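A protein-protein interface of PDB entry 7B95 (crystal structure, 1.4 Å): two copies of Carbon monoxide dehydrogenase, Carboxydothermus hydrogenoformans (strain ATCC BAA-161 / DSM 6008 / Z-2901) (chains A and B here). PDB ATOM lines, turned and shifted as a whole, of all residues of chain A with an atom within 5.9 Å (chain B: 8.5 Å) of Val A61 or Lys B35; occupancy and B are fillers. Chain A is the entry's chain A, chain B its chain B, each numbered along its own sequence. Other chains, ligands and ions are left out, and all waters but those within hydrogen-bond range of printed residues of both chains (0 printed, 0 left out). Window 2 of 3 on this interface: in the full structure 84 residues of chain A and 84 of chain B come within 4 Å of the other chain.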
ATOM      1  N   ASN A  58      28.483  23.262 -15.805  1.00  0.00           N
ATOM      2  CA  ASN A  58      27.965  22.340 -14.793  1.00  0.00           C
ATOM      3  C   ASN A  58      27.452  21.121 -15.541  1.00  0.00           C
ATOM      4  O   ASN A  58      26.343  21.148 -16.052  1.00  0.00           O
ATOM      5  CB  ASN A  58      26.878  23.013 -13.960  1.00  0.00           C
ATOM      6  CG  ASN A  58      26.372  22.121 -12.856  1.00  0.00           C
ATOM      7  OD1 ASN A  58      26.407  20.892 -12.978  1.00  0.00           O
ATOM      8  ND2 ASN A  58      25.925  22.723 -11.760  1.00  0.00           N
ATOM      9  N   GLU A  59      28.252  20.046 -15.572  1.00  0.00           N
ATOM     10  CA  GLU A  59      27.872  18.889 -16.379  1.00  0.00           C
ATOM     11  C   GLU A  59      26.618  18.220 -15.842  1.00  0.00           C
ATOM     12  O   GLU A  59      25.889  17.580 -16.607  1.00  0.00           O
ATOM     13  CB  GLU A  59      29.046  17.908 -16.484  1.00  0.00           C
ATOM     14  CG  GLU A  59      30.287  18.610 -17.045  1.00  0.00           C
ATOM     15  CD  GLU A  59      31.284  17.686 -17.714  1.00  0.00           C
ATOM     16  OE1 GLU A  59      32.424  18.135 -17.949  1.00  0.00           O
ATOM     17  OE2 GLU A  59      30.933  16.523 -18.009  1.00  0.00           O
ATOM     18  N   LYS A  60      26.348  18.366 -14.548  1.00  0.00           N
ATOM     19  CA  LYS A  60      25.223  17.672 -13.930  1.00  0.00           C
ATOM     20  C   LYS A  60      23.875  18.211 -14.393  1.00  0.00           C
ATOM     21  O   LYS A  60      22.869  17.504 -14.247  1.00  0.00           O
ATOM     22  CB  LYS A  60      25.318  17.750 -12.404  1.00  0.00           C
ATOM     23  CG  LYS A  60      26.460  16.963 -11.760  1.00  0.00           C
ATOM     24  CD  LYS A  60      26.413  17.163 -10.234  1.00  0.00           C
ATOM     25  CE  LYS A  60      27.582  16.537  -9.498  1.00  0.00           C
ATOM     26  NZ  LYS A  60      27.679  15.080  -9.732  1.00  0.00           N
ATOM     27  N   VAL A  61      23.820  19.424 -14.947  1.00  0.00           N
ATOM     28  CA  VAL A  61      22.615  19.957 -15.564  1.00  0.00           C
ATOM     29  C   VAL A  61      22.728  20.057 -17.078  1.00  0.00           C
ATOM     30  O   VAL A  61      21.862  20.682 -17.725  1.00  0.00           O
ATOM     31  CB  VAL A  61      22.182  21.292 -14.939  1.00  0.00           C
ATOM     32  CG1 VAL A  61      22.063  21.152 -13.438  1.00  0.00           C
ATOM     33  CG2 VAL A  61      23.160  22.410 -15.291  1.00  0.00           C
ATOM     34  N   GLY A  62      23.739  19.440 -17.676  1.00  0.00           N
ATOM     35  CA  GLY A  62      23.879  19.431 -19.116  1.00  0.00           C
ATOM     36  C   GLY A  62      24.639  20.605 -19.680  1.00  0.00           C
ATOM     37  O   GLY A  62      24.742  20.735 -20.909  1.00  0.00           O
ATOM     38  N   ALA A  63      25.184  21.462 -18.821  1.00  0.00           N
ATOM     39  CA  ALA A  63      25.945  22.630 -19.247  1.00  0.00           C
ATOM     40  C   ALA A  63      27.430  22.279 -19.324  1.00  0.00           C
ATOM     41  O   ALA A  63      28.237  22.678 -18.501  1.00  0.00           O
ATOM     42  CB  ALA A  63      25.696  23.782 -18.291  1.00  0.00           C
ATOM     43  N   ARG B  29      23.181  24.538 -27.133  1.00  0.00           N
ATOM     44  CA  ARG B  29      23.928  24.830 -25.916  1.00  0.00           C
ATOM     45  C   ARG B  29      23.352  26.002 -25.136  1.00  0.00           C
ATOM     46  O   ARG B  29      23.662  26.146 -23.949  1.00  0.00           O
ATOM     47  CB  ARG B  29      25.406  25.109 -26.238  1.00  0.00           C
ATOM     48  CG  ARG B  29      26.201  23.904 -26.641  1.00  0.00           C
ATOM     49  CD  ARG B  29      27.669  24.178 -26.779  1.00  0.00           C
ATOM     50  NE  ARG B  29      27.976  25.162 -27.809  1.00  0.00           N
ATOM     51  CZ  ARG B  29      28.410  24.852 -29.033  1.00  0.00           C
ATOM     52  NH1 ARG B  29      28.542  23.577 -29.413  1.00  0.00           N
ATOM     53  NH2 ARG B  29      28.685  25.819 -29.891  1.00  0.00           N
ATOM     54  N   PHE B  30      22.503  26.819 -25.757  1.00  0.00           N
ATOM     55  CA  PHE B  30      21.874  27.912 -25.028  1.00  0.00           C
ATOM     56  C   PHE B  30      20.969  27.375 -23.921  1.00  0.00           C
ATOM     57  O   PHE B  30      20.904  27.949 -22.827  1.00  0.00           O
ATOM     58  CB  PHE B  30      21.080  28.779 -26.014  1.00  0.00           C
ATOM     59  CG  PHE B  30      20.751  30.143 -25.505  1.00  0.00           C
ATOM     60  CD1 PHE B  30      21.601  31.208 -25.733  1.00  0.00           C
ATOM     61  CD2 PHE B  30      19.557  30.395 -24.875  1.00  0.00           C
ATOM     62  CE1 PHE B  30      21.306  32.458 -25.266  1.00  0.00           C
ATOM     63  CE2 PHE B  30      19.260  31.672 -24.422  1.00  0.00           C
ATOM     64  CZ  PHE B  30      20.100  32.699 -24.636  1.00  0.00           C
ATOM     65  N   ASP B  31      20.297  26.247 -24.180  1.00  0.00           N
ATOM     66  CA  ASP B  31      19.240  25.784 -23.280  1.00  0.00           C
ATOM     67  C   ASP B  31      19.757  25.355 -21.915  1.00  0.00           C
ATOM     68  O   ASP B  31      19.191  25.791 -20.896  1.00  0.00           O
ATOM     69  CB  ASP B  31      18.385  24.713 -23.975  1.00  0.00           C
ATOM     70  CG  ASP B  31      17.626  25.256 -25.153  1.00  0.00           C
ATOM     71  OD1 ASP B  31      17.298  26.463 -25.146  1.00  0.00           O
ATOM     72  OD2 ASP B  31      17.344  24.474 -26.090  1.00  0.00           O
ATOM     73  N   PRO B  32      20.820  24.569 -21.797  1.00  0.00           N
ATOM     74  CA  PRO B  32      21.300  24.265 -20.444  1.00  0.00           C
ATOM     75  C   PRO B  32      21.737  25.489 -19.680  1.00  0.00           C
ATOM     76  O   PRO B  32      21.587  25.518 -18.458  1.00  0.00           O
ATOM     77  CB  PRO B  32      22.436  23.265 -20.674  1.00  0.00           C
ATOM     78  CG  PRO B  32      22.166  22.690 -22.028  1.00  0.00           C
ATOM     79  CD  PRO B  32      21.542  23.791 -22.816  1.00  0.00           C
ATOM     80  N   GLN B  33      22.308  26.493 -20.354  1.00  0.00           N
ATOM     81  CA  GLN B  33      22.722  27.690 -19.637  1.00  0.00           C
ATOM     82  C   GLN B  33      21.518  28.391 -19.020  1.00  0.00           C
ATOM     83  O   GLN B  33      21.630  28.995 -17.944  1.00  0.00           O
ATOM     84  CB  GLN B  33      23.417  28.643 -20.615  1.00  0.00           C
ATOM     85  CG  GLN B  33      24.743  28.123 -21.147  1.00  0.00           C
ATOM     86  CD  GLN B  33      25.785  27.929 -20.055  1.00  0.00           C
ATOM     87  OE1 GLN B  33      25.770  28.628 -19.026  1.00  0.00           O
ATOM     88  NE2 GLN B  33      26.693  26.976 -20.257  1.00  0.00           N
ATOM     89  N   GLU B  34      20.366  28.305 -19.683  1.00  0.00           N
ATOM     90  CA  GLU B  34      19.152  28.931 -19.163  1.00  0.00           C
ATOM     91  C   GLU B  34      18.692  28.326 -17.841  1.00  0.00           C
ATOM     92  O   GLU B  34      17.862  28.940 -17.153  1.00  0.00           O
ATOM     93  CB  GLU B  34      18.036  28.856 -20.203  1.00  0.00           C
ATOM     94  CG  GLU B  34      18.262  29.811 -21.368  1.00  0.00           C
ATOM     95  CD  GLU B  34      18.170  31.249 -20.936  1.00  0.00           C
ATOM     96  OE1 GLU B  34      17.048  31.700 -20.630  1.00  0.00           O
ATOM     97  OE2 GLU B  34      19.184  31.948 -20.908  1.00  0.00           O
ATOM     98  N   LYS B  35      19.183  27.143 -17.467  1.00  0.00           N
ATOM     99  CA  LYS B  35      18.761  26.529 -16.209  1.00  0.00           C
ATOM    100  C   LYS B  35      19.381  27.193 -14.999  1.00  0.00           C
ATOM    101  O   LYS B  35      18.800  27.120 -13.902  1.00  0.00           O
ATOM    102  CB  LYS B  35      19.194  25.064 -16.204  1.00  0.00           C
ATOM    103  CG  LYS B  35      18.534  24.206 -17.273  1.00  0.00           C
ATOM    104  CD  LYS B  35      19.092  22.799 -17.170  1.00  0.00           C
ATOM    105  CE  LYS B  35      18.510  21.876 -18.196  1.00  0.00           C
ATOM    106  NZ  LYS B  35      19.041  20.503 -18.034  1.00  0.00           N
ATOM    107  N   ILE B  36      20.548  27.844 -15.164  1.00  0.00           N
ATOM    108  CA  ILE B  36      21.373  28.242 -14.022  1.00  0.00           C
ATOM    109  C   ILE B  36      21.977  29.631 -14.213  1.00  0.00           C
ATOM    110  O   ILE B  36      23.055  29.921 -13.677  1.00  0.00           O
ATOM    111  CB  ILE B  36      22.469  27.196 -13.727  1.00  0.00           C
ATOM    112  CG1 ILE B  36      23.368  26.959 -14.947  1.00  0.00           C
ATOM    113  CG2 ILE B  36      21.843  25.885 -13.248  1.00  0.00           C
ATOM    114  CD1 ILE B  36      24.609  26.092 -14.687  1.00  0.00           C
ATOM    115  N   ARG B  37      21.290  30.526 -14.941  1.00  0.00           N
ATOM    116  CA  ARG B  37      21.843  31.859 -15.194  1.00  0.00           C
ATOM    117  C   ARG B  37      22.089  32.645 -13.905  1.00  0.00           C
ATOM    118  O   ARG B  37      21.286  32.630 -12.968  1.00  0.00           O
ATOM    119  CB  ARG B  37      20.925  32.697 -16.091  1.00  0.00           C
ATOM    120  CG  ARG B  37      20.780  32.224 -17.524  1.00  0.00           C
ATOM    121  CD  ARG B  37      22.055  32.291 -18.352  1.00  0.00           C
ATOM    122  NE  ARG B  37      21.697  32.115 -19.746  1.00  0.00           N
ATOM    123  CZ  ARG B  37      22.538  32.266 -20.764  1.00  0.00           C
ATOM    124  NH1 ARG B  37      22.102  32.132 -22.009  1.00  0.00           N
ATOM    125  NH2 ARG B  37      23.816  32.513 -20.542  1.00  0.00           N
ATOM    126  N   CYS B  38      23.210  33.368 -13.897  1.00  0.00           N
ATOM    127  CA  CYS B  38      23.586  34.259 -12.808  1.00  0.00           C
ATOM    128  C   CYS B  38      23.077  35.669 -13.079  1.00  0.00           C
ATOM    129  O   CYS B  38      23.577  36.348 -13.978  1.00  0.00           O
ATOM    130  CB  CYS B  38      25.106  34.286 -12.655  1.00  0.00           C
ATOM    131  SG  CYS B  38      25.599  35.390 -11.355  1.00  0.00           S
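CD1 of Ile B36 touches CB of Asn A58, at 3.9 Å. Val A61 touches Pro B32. Pro B32 touches Gly A62. Pro B32 touches Ala A63. Gln B33 touches Ala A63.
N of Lys A60 is in hydrogen-bond range of OD1 of Asn A58, at 3.0 Å. The backbone NH (N) of Asn A58 lies within hydrogen-bond range of the backbone carbonyl oxygen (O) of Ala A63, at 2.8 Å.
Along chain B the printed residues that touch a printed residue of chain A span positions 32 to 36. Of the 6 printed residues of chain A, 4 touch a printed residue of chain B. Printed residues of chain A that touch a printed residue of chain B: Asn A58, Val A61, Gly A62 and Ala A63. Among the printed residues, 6 pairs touch across the chains.
No position is printed for both chains.
Printed residues of chain B within 4 Å of Val A61: Pro B32 (3.96 Å) and Lys B35 (2.8 Å). Lys B35 touches just one residue of chain A: Val A61 (2.8 Å). Of the printed residues of chain B, Gly A62 touches Pro B32. Of the printed residues of chain A, Pro B32 touches Val A61, Gly A62 and Ala A63. Printed residues of chain A within 4 Å of Gln B33: Ala A63. Of the printed residues of chain B, Asn A58 touches Ile B36. Of the printed residues of chain A, Ile B36 touches Asn A58 (3.9 Å). Printed residues of chain B within 4 Å of Ala A63: Pro B32 and Gln B33. Arg B29 touches none of the printed residues of chain A. The nearest printed residue of chain B that does not touch Val A61 is Ile B36 (4.003 Å). The nearest printed residue of chain A that does not touch Ile B36 is Val A61 (4.003 Å).
The backbone carbonyl oxygen (O) of Val A61 sits at hydrogen-bond distance from the side-chain amino group (NZ) of Lys B35 (2.8 Å).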
